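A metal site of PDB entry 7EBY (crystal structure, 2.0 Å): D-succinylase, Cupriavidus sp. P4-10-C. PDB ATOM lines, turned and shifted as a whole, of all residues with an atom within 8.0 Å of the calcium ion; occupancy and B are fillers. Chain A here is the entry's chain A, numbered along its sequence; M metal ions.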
ATOM      1  N   LEU A 184     -27.916  -2.084 -28.590  1.00  0.00           N
ATOM      2  CA  LEU A 184     -28.100  -3.083 -27.547  1.00  0.00           C
ATOM      3  C   LEU A 184     -27.676  -4.404 -28.183  1.00  0.00           C
ATOM      4  O   LEU A 184     -27.573  -4.487 -29.414  1.00  0.00           O
ATOM      5  CB  LEU A 184     -29.566  -3.122 -27.023  1.00  0.00           C
ATOM      6  CG  LEU A 184     -30.608  -3.890 -27.849  1.00  0.00           C
ATOM      7  CD1 LEU A 184     -31.908  -4.037 -27.073  1.00  0.00           C
ATOM      8  CD2 LEU A 184     -30.881  -3.173 -29.177  1.00  0.00           C
ATOM      9  N   ASN A 185     -27.409  -5.435 -27.368  1.00  0.00           N
ATOM     10  CA  ASN A 185     -27.637  -5.450 -25.932  1.00  0.00           C
ATOM     11  C   ASN A 185     -26.455  -5.937 -25.109  1.00  0.00           C
ATOM     12  O   ASN A 185     -26.634  -6.777 -24.229  1.00  0.00           O
ATOM     13  CB  ASN A 185     -28.867  -6.320 -25.591  1.00  0.00           C
ATOM     14  CG  ASN A 185     -28.664  -7.809 -25.927  1.00  0.00           C
ATOM     15  OD1 ASN A 185     -27.748  -8.185 -26.670  1.00  0.00           O
ATOM     16  ND2 ASN A 185     -29.503  -8.660 -25.337  1.00  0.00           N
ATOM     17  N   PHE A 186     -25.262  -5.383 -25.354  1.00  0.00           N
ATOM     18  CA  PHE A 186     -24.121  -5.705 -24.491  1.00  0.00           C
ATOM     19  C   PHE A 186     -24.474  -5.545 -23.024  1.00  0.00           C
ATOM     20  O   PHE A 186     -24.154  -6.415 -22.194  1.00  0.00           O
ATOM     21  CB  PHE A 186     -22.926  -4.819 -24.847  1.00  0.00           C
ATOM     22  CG  PHE A 186     -21.910  -4.714 -23.729  1.00  0.00           C
ATOM     23  CD1 PHE A 186     -20.879  -5.640 -23.609  1.00  0.00           C
ATOM     24  CD2 PHE A 186     -22.000  -3.687 -22.785  1.00  0.00           C
ATOM     25  CE1 PHE A 186     -19.953  -5.538 -22.575  1.00  0.00           C
ATOM     26  CE2 PHE A 186     -21.074  -3.591 -21.738  1.00  0.00           C
ATOM     27  CZ  PHE A 186     -20.059  -4.497 -21.641  1.00  0.00           C
ATOM     28  N   THR A 187     -25.107  -4.438 -22.662  1.00  0.00           N
ATOM     29  CA  THR A 187     -25.414  -4.217 -21.254  1.00  0.00           C
ATOM     30  C   THR A 187     -26.365  -5.284 -20.740  1.00  0.00           C
ATOM     31  O   THR A 187     -26.171  -5.802 -19.633  1.00  0.00           O
ATOM     32  CB  THR A 187     -25.998  -2.828 -21.056  1.00  0.00           C
ATOM     33  OG1 THR A 187     -25.096  -1.865 -21.615  1.00  0.00           O
ATOM     34  CG2 THR A 187     -26.196  -2.552 -19.580  1.00  0.00           C
ATOM     35  N   GLY A 188     -27.378  -5.631 -21.524  1.00  0.00           N
ATOM     36  CA  GLY A 188     -28.308  -6.673 -21.115  1.00  0.00           C
ATOM     37  C   GLY A 188     -27.667  -8.032 -20.969  1.00  0.00           C
ATOM     38  O   GLY A 188     -27.938  -8.770 -20.013  1.00  0.00           O
ATOM     39  N   GLU A 189     -26.798  -8.394 -21.929  1.00  0.00           N
ATOM     40  CA  GLU A 189     -26.071  -9.658 -21.812  1.00  0.00           C
ATOM     41  C   GLU A 189     -25.268  -9.694 -20.529  1.00  0.00           C
ATOM     42  O   GLU A 189     -25.270 -10.695 -19.805  1.00  0.00           O
ATOM     43  CB  GLU A 189     -25.139  -9.843 -23.020  1.00  0.00           C
ATOM     44  CG  GLU A 189     -25.814 -10.032 -24.341  1.00  0.00           C
ATOM     45  CD  GLU A 189     -24.823 -10.378 -25.442  1.00  0.00           C
ATOM     46  OE1 GLU A 189     -23.639 -10.562 -25.119  1.00  0.00           O
ATOM     47  OE2 GLU A 189     -25.223 -10.457 -26.641  1.00  0.00           O
ATOM     48  N   ARG A 192     -27.652  -9.962 -17.535  1.00  0.00           N
ATOM     49  CA  ARG A 192     -28.310 -11.273 -17.468  1.00  0.00           C
ATOM     50  C   ARG A 192     -27.337 -12.373 -17.030  1.00  0.00           C
ATOM     51  O   ARG A 192     -27.691 -13.224 -16.207  1.00  0.00           O
ATOM     52  CB  ARG A 192     -28.960 -11.609 -18.822  1.00  0.00           C
ATOM     53  CG  ARG A 192     -29.753 -12.909 -18.803  1.00  0.00           C
ATOM     54  CD  ARG A 192     -30.596 -13.146 -20.065  1.00  0.00           C
ATOM     55  NE  ARG A 192     -31.777 -12.307 -20.112  1.00  0.00           N
ATOM     56  CZ  ARG A 192     -31.892 -11.240 -20.883  1.00  0.00           C
ATOM     57  NH1 ARG A 192     -30.918 -10.871 -21.698  1.00  0.00           N
ATOM     58  NH2 ARG A 192     -33.004 -10.519 -20.820  1.00  0.00           N
ATOM     59  N   MET A 353     -33.332  -4.365 -33.126  1.00  0.00           N
ATOM     60  CA  MET A 353     -32.506  -5.481 -33.563  1.00  0.00           C
ATOM     61  C   MET A 353     -31.316  -5.598 -32.635  1.00  0.00           C
ATOM     62  O   MET A 353     -30.679  -4.598 -32.288  1.00  0.00           O
ATOM     63  CB  MET A 353     -31.964  -5.299 -34.978  1.00  0.00           C
ATOM     64  CG  MET A 353     -32.975  -5.089 -35.991  1.00  0.00           C
ATOM     65  SD  MET A 353     -32.786  -3.413 -36.526  1.00  0.00           S
ATOM     66  CE  MET A 353     -33.934  -3.514 -37.880  1.00  0.00           C
ATOM     67  N   ASP A 354     -31.000  -6.819 -32.256  1.00  0.00           N
ATOM     68  CA  ASP A 354     -29.885  -7.075 -31.372  1.00  0.00           C
ATOM     69  C   ASP A 354     -28.592  -6.920 -32.168  1.00  0.00           C
ATOM     70  O   ASP A 354     -28.274  -7.757 -33.033  1.00  0.00           O
ATOM     71  CB  ASP A 354     -30.045  -8.449 -30.745  1.00  0.00           C
ATOM     72  CG  ASP A 354     -28.816  -8.890 -29.972  1.00  0.00           C
ATOM     73  OD1 ASP A 354     -27.843  -8.111 -29.841  1.00  0.00           O
ATOM     74  OD2 ASP A 354     -28.864 -10.018 -29.441  1.00  0.00           O
ATOM     75  N   GLN A 355     -27.839  -5.849 -31.892  1.00  0.00           N
ATOM     76  CA  GLN A 355     -26.664  -5.514 -32.694  1.00  0.00           C
ATOM     77  C   GLN A 355     -25.354  -5.583 -31.908  1.00  0.00           C
ATOM     78  O   GLN A 355     -24.319  -5.140 -32.430  1.00  0.00           O
ATOM     79  CB  GLN A 355     -26.858  -4.140 -33.331  1.00  0.00           C
ATOM     80  CG  GLN A 355     -27.924  -4.133 -34.463  1.00  0.00           C
ATOM     81  CD  GLN A 355     -28.197  -2.763 -35.078  1.00  0.00           C
ATOM     82  OE1 GLN A 355     -27.978  -1.730 -34.450  1.00  0.00           O
ATOM     83  NE2 GLN A 355     -28.658  -2.772 -36.324  1.00  0.00           N
ATOM     84  N   GLU A 356     -25.348  -6.174 -30.715  1.00  0.00           N
ATOM     85  CA  GLU A 356     -24.125  -6.327 -29.926  1.00  0.00           C
ATOM     86  C   GLU A 356     -24.133  -7.667 -29.225  1.00  0.00           C
ATOM     87  O   GLU A 356     -25.074  -7.979 -28.486  1.00  0.00           O
ATOM     88  CB  GLU A 356     -23.995  -5.242 -28.851  1.00  0.00           C
ATOM     89  CG  GLU A 356     -23.882  -3.833 -29.339  1.00  0.00           C
ATOM     90  CD  GLU A 356     -23.896  -2.831 -28.199  1.00  0.00           C
ATOM     91  OE1 GLU A 356     -24.738  -2.977 -27.296  1.00  0.00           O
ATOM     92  OE2 GLU A 356     -23.073  -1.886 -28.225  1.00  0.00           O
ATOM     93  N   ASP A 357     -23.059  -8.427 -29.381  1.00  0.00           N
ATOM     94  CA  ASP A 357     -22.836  -9.635 -28.595  1.00  0.00           C
ATOM     95  C   ASP A 357     -21.500  -9.538 -27.884  1.00  0.00           C
ATOM     96  O   ASP A 357     -20.499  -9.099 -28.478  1.00  0.00           O
ATOM     97  CB  ASP A 357     -22.859 -10.876 -29.492  1.00  0.00           C
ATOM     98  CG  ASP A 357     -24.234 -11.162 -30.075  1.00  0.00           C
ATOM     99  OD1 ASP A 357     -25.244 -10.589 -29.601  1.00  0.00           O
ATOM    100  OD2 ASP A 357     -24.306 -11.990 -31.001  1.00  0.00           O
ATOM    101  N   LEU A 358     -21.470  -9.977 -26.634  1.00  0.00           N
ATOM    102  CA  LEU A 358     -20.214 -10.073 -25.921  1.00  0.00           C
ATOM    103  C   LEU A 358     -19.608 -11.451 -26.168  1.00  0.00           C
ATOM    104  O   LEU A 358     -20.281 -12.471 -25.968  1.00  0.00           O
ATOM    105  CB  LEU A 358     -20.402  -9.848 -24.428  1.00  0.00           C
ATOM    106  CG  LEU A 358     -19.119  -9.959 -23.598  1.00  0.00           C
ATOM    107  CD1 LEU A 358     -18.170  -8.880 -24.014  1.00  0.00           C
ATOM    108  CD2 LEU A 358     -19.464  -9.811 -22.128  1.00  0.00           C
ATOM    109  N   ARG A 422     -18.451  -7.766 -29.976  1.00  0.00           N
ATOM    110  CA  ARG A 422     -18.820  -7.946 -31.366  1.00  0.00           C
ATOM    111  C   ARG A 422     -20.010  -7.033 -31.636  1.00  0.00           C
ATOM    112  O   ARG A 422     -21.163  -7.367 -31.311  1.00  0.00           O
ATOM    113  CB  ARG A 422     -19.115  -9.407 -31.700  1.00  0.00           C
ATOM    114  CG  ARG A 422     -19.162  -9.607 -33.217  1.00  0.00           C
ATOM    115  CD  ARG A 422     -19.382 -11.095 -33.625  1.00  0.00           C
ATOM    116  NE  ARG A 422     -19.191 -11.279 -35.062  1.00  0.00           N
ATOM    117  CZ  ARG A 422     -19.151 -12.464 -35.674  1.00  0.00           C
ATOM    118  NH1 ARG A 422     -19.335 -13.594 -35.011  1.00  0.00           N
ATOM    119  NH2 ARG A 422     -18.957 -12.505 -36.987  1.00  0.00           N
ATOM    120  N   VAL A 480     -28.535  -9.126 -37.516  1.00  0.00           N
ATOM    121  CA  VAL A 480     -27.628 -10.242 -37.330  1.00  0.00           C
ATOM    122  C   VAL A 480     -28.398 -11.558 -37.372  1.00  0.00           C
ATOM    123  O   VAL A 480     -29.476 -11.685 -36.782  1.00  0.00           O
ATOM    124  CB  VAL A 480     -26.901 -10.097 -35.975  1.00  0.00           C
ATOM    125  CG1 VAL A 480     -26.101 -11.332 -35.686  1.00  0.00           C
ATOM    126  CG2 VAL A 480     -26.027  -8.863 -35.955  1.00  0.00           C
ATOM    127  N   ARG A 482     -28.148 -15.232 -36.002  1.00  0.00           N
ATOM    128  CA  ARG A 482     -27.510 -16.107 -35.031  1.00  0.00           C
ATOM    129  C   ARG A 482     -28.139 -17.484 -35.186  1.00  0.00           C
ATOM    130  O   ARG A 482     -29.244 -17.727 -34.684  1.00  0.00           O
ATOM    131  CB  ARG A 482     -27.703 -15.579 -33.608  1.00  0.00           C
ATOM    132  CG  ARG A 482     -27.091 -14.190 -33.356  1.00  0.00           C
ATOM    133  CD  ARG A 482     -27.448 -13.641 -31.959  1.00  0.00           C
ATOM    134  NE  ARG A 482     -26.903 -12.297 -31.741  1.00  0.00           N
ATOM    135  CZ  ARG A 482     -27.453 -11.169 -32.172  1.00  0.00           C
ATOM    136  NH1 ARG A 482     -28.612 -11.164 -32.811  1.00  0.00           N
ATOM    137  NH2 ARG A 482     -26.809 -10.020 -31.993  1.00  0.00           N
ATOM    138  N   TRP A 485     -27.916 -19.381 -31.209  1.00  0.00           N
ATOM    139  CA  TRP A 485     -28.096 -18.804 -29.872  1.00  0.00           C
ATOM    140  C   TRP A 485     -28.998 -17.583 -29.997  1.00  0.00           C
ATOM    141  O   TRP A 485     -29.192 -17.046 -31.096  1.00  0.00           O
ATOM    142  CB  TRP A 485     -26.768 -18.481 -29.180  1.00  0.00           C
ATOM    143  CG  TRP A 485     -26.030 -17.228 -29.580  1.00  0.00           C
ATOM    144  CD1 TRP A 485     -25.905 -16.091 -28.830  1.00  0.00           C
ATOM    145  CD2 TRP A 485     -25.281 -16.995 -30.775  1.00  0.00           C
ATOM    146  NE1 TRP A 485     -25.126 -15.173 -29.483  1.00  0.00           N
ATOM    147  CE2 TRP A 485     -24.745 -15.696 -30.684  1.00  0.00           C
ATOM    148  CE3 TRP A 485     -25.021 -17.761 -31.917  1.00  0.00           C
ATOM    149  CZ2 TRP A 485     -23.965 -15.132 -31.705  1.00  0.00           C
ATOM    150  CZ3 TRP A 485     -24.240 -17.202 -32.925  1.00  0.00           C
ATOM    151  CH2 TRP A 485     -23.726 -15.904 -32.811  1.00  0.00           C
ATOM    152  N   ASP A 486     -29.589 -17.175 -28.867  1.00  0.00           N
ATOM    153  CA  ASP A 486     -30.628 -16.147 -28.896  1.00  0.00           C
ATOM    154  C   ASP A 486     -30.109 -14.740 -28.628  1.00  0.00           C
ATOM    155  O   ASP A 486     -30.910 -13.801 -28.536  1.00  0.00           O
ATOM    156  CB  ASP A 486     -31.756 -16.469 -27.913  1.00  0.00           C
ATOM    157  CG  ASP A 486     -31.279 -16.644 -26.492  1.00  0.00           C
ATOM    158  OD1 ASP A 486     -30.177 -16.140 -26.157  1.00  0.00           O
ATOM    159  OD2 ASP A 486     -32.040 -17.220 -25.692  1.00  0.00           O
ATOM    160  N   GLY A 487     -28.791 -14.569 -28.447  1.00  0.00           N
ATOM    161  CA  GLY A 487     -28.185 -13.265 -28.277  1.00  0.00           C
ATOM    162  C   GLY A 487     -28.474 -12.551 -26.972  1.00  0.00           C
ATOM    163  O   GLY A 487     -28.106 -11.392 -26.839  1.00  0.00           O
ATOM    164  N   LEU A 488     -29.111 -13.222 -26.007  1.00  0.00           N
ATOM    165  CA  LEU A 488     -29.426 -12.640 -24.704  1.00  0.00           C
ATOM    166  C   LEU A 488     -28.356 -12.900 -23.667  1.00  0.00           C
ATOM    167  O   LEU A 488     -28.458 -12.379 -22.540  1.00  0.00           O
ATOM    168  CB  LEU A 488     -30.775 -13.168 -24.192  1.00  0.00           C
ATOM    169  CG  LEU A 488     -31.980 -12.933 -25.092  1.00  0.00           C
ATOM    170  CD1 LEU A 488     -33.160 -13.764 -24.581  1.00  0.00           C
ATOM    171  CD2 LEU A 488     -32.353 -11.461 -25.200  1.00  0.00           C
ATOM    172  N   PHE A 489     -27.360 -13.725 -23.989  1.00  0.00           N
ATOM    173  CA  PHE A 489     -26.200 -13.999 -23.158  1.00  0.00           C
ATOM    174  C   PHE A 489     -24.933 -13.785 -23.967  1.00  0.00           C
ATOM    175  O   PHE A 489     -24.958 -13.844 -25.201  1.00  0.00           O
ATOM    176  CB  PHE A 489     -26.205 -15.442 -22.648  1.00  0.00           C
ATOM    177  CG  PHE A 489     -27.297 -15.792 -21.669  1.00  0.00           C
ATOM    178  CD1 PHE A 489     -27.139 -15.512 -20.318  1.00  0.00           C
ATOM    179  CD2 PHE A 489     -28.428 -16.477 -22.097  1.00  0.00           C
ATOM    180  CE1 PHE A 489     -28.122 -15.867 -19.412  1.00  0.00           C
ATOM    181  CE2 PHE A 489     -29.404 -16.834 -21.184  1.00  0.00           C
ATOM    182  CZ  PHE A 489     -29.263 -16.516 -19.847  1.00  0.00           C
ATOM    183  N   PRO A 490     -23.797 -13.555 -23.296  1.00  0.00           N
ATOM    184  CA  PRO A 490     -22.501 -13.677 -23.981  1.00  0.00           C
ATOM    185  C   PRO A 490     -22.279 -15.089 -24.492  1.00  0.00           C
ATOM    186  O   PRO A 490     -22.839 -16.064 -23.974  1.00  0.00           O
ATOM    187  CB  PRO A 490     -21.479 -13.331 -22.890  1.00  0.00           C
ATOM    188  CG  PRO A 490     -22.280 -12.518 -21.875  1.00  0.00           C
ATOM    189  CD  PRO A 490     -23.659 -13.088 -21.903  1.00  0.00           C
ATOM    190  N   TRP A 499     -21.991 -15.241 -36.250  1.00  0.00           N
ATOM    191  CA  TRP A 499     -22.983 -14.612 -37.091  1.00  0.00           C
ATOM    192  C   TRP A 499     -22.925 -15.262 -38.458  1.00  0.00           C
ATOM    193  O   TRP A 499     -21.848 -15.556 -38.983  1.00  0.00           O
ATOM    194  CB  TRP A 499     -22.706 -13.101 -37.206  1.00  0.00           C
ATOM    195  CG  TRP A 499     -22.842 -12.334 -35.896  1.00  0.00           C
ATOM    196  CD1 TRP A 499     -23.212 -12.834 -34.674  1.00  0.00           C
ATOM    197  CD2 TRP A 499     -22.620 -10.928 -35.700  1.00  0.00           C
ATOM    198  NE1 TRP A 499     -23.237 -11.824 -33.731  1.00  0.00           N
ATOM    199  CE2 TRP A 499     -22.874 -10.639 -34.341  1.00  0.00           C
ATOM    200  CE3 TRP A 499     -22.237  -9.870 -36.543  1.00  0.00           C
ATOM    201  CZ2 TRP A 499     -22.754  -9.364 -33.808  1.00  0.00           C
ATOM    202  CZ3 TRP A 499     -22.117  -8.596 -36.010  1.00  0.00           C
ATOM    203  CH2 TRP A 499     -22.368  -8.358 -34.657  1.00  0.00           C
ATOM    204  N   GLU A 541     -35.750  -7.834 -26.745  1.00  0.00           N
ATOM    205  CA  GLU A 541     -35.792  -6.828 -25.695  1.00  0.00           C
ATOM    206  C   GLU A 541     -36.264  -5.534 -26.317  1.00  0.00           C
ATOM    207  O   GLU A 541     -35.532  -4.858 -27.051  1.00  0.00           O
ATOM    208  CB  GLU A 541     -34.424  -6.672 -25.013  1.00  0.00           C
ATOM    209  CG  GLU A 541     -34.012  -7.941 -24.256  1.00  0.00           C
ATOM    210  CD  GLU A 541     -32.593  -7.875 -23.736  1.00  0.00           C
ATOM    211  OE1 GLU A 541     -31.743  -7.274 -24.427  1.00  0.00           O
ATOM    212  OE2 GLU A 541     -32.326  -8.435 -22.649  1.00  0.00           O
HETATM  213 CA    CA M   1     -26.835  -9.741 -28.068  1.00  0.00          CA
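The side-chain carboxylate (OE1) of Glu 189 lies within hydrogen-bond range of the backbone NH (N) of Leu 358 (2.7 Å).
The side-chain amide nitrogen (ND2) of Asn 185 is in hydrogen-bond range of the side-chain carboxylate (OE1) of Glu 541.
OD2 of Asp 357 is in salt-bridge range of NE of Arg 482.
O of Asp 357 lies within hydrogen-bond range of N of Arg 422, at 2.9 Å.
The side-chain carboxylate of Asp 357 is in hydrogen-bond range of the indole nitrogen of Trp 499 (2.9 Å).
The backbone carbonyl oxygen of Asp 354 sits at hydrogen-bond distance from the guanidinium group of Arg 482 (2.9 Å).
The side-chain carboxylate (OE1) of Glu 356 is in hydrogen-bond range of the backbone NH (N) of Phe 186, 3.1 Å away.
The backbone NH (N) of Glu 356 sits at hydrogen-bond distance from the backbone carbonyl oxygen (O) of Leu 184 (3.1 Å).
The calcium ion is bound by the side-chain carboxylate (OE2) of Glu 189, at 2.3 Å.
The side-chain amide oxygen (OD1) of Asn 185 binds the calcium ion (2.3 Å).
The side-chain carboxylate (OD1) of Asp 357 binds the calcium ion (2.4 Å).
O of Gly 487 is bound to the calcium ion (2.4 Å).
OD2 of Asp 354 is bound to the calcium ion, at 2.5 Å.
The calcium ion is bound by the backbone carbonyl oxygen (O) of Glu 356 (2.5 Å).
The calcium ion is bound by OD1 of Asp 354.
The calcium ion has seven donor atoms within binding distance.
Arg 482 touches the calcium ion.
Within 4 Å of the calcium ion: Asn 185, Glu 189, Asp 354, Glu 356, Asp 357, Arg 482 and Gly 487.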
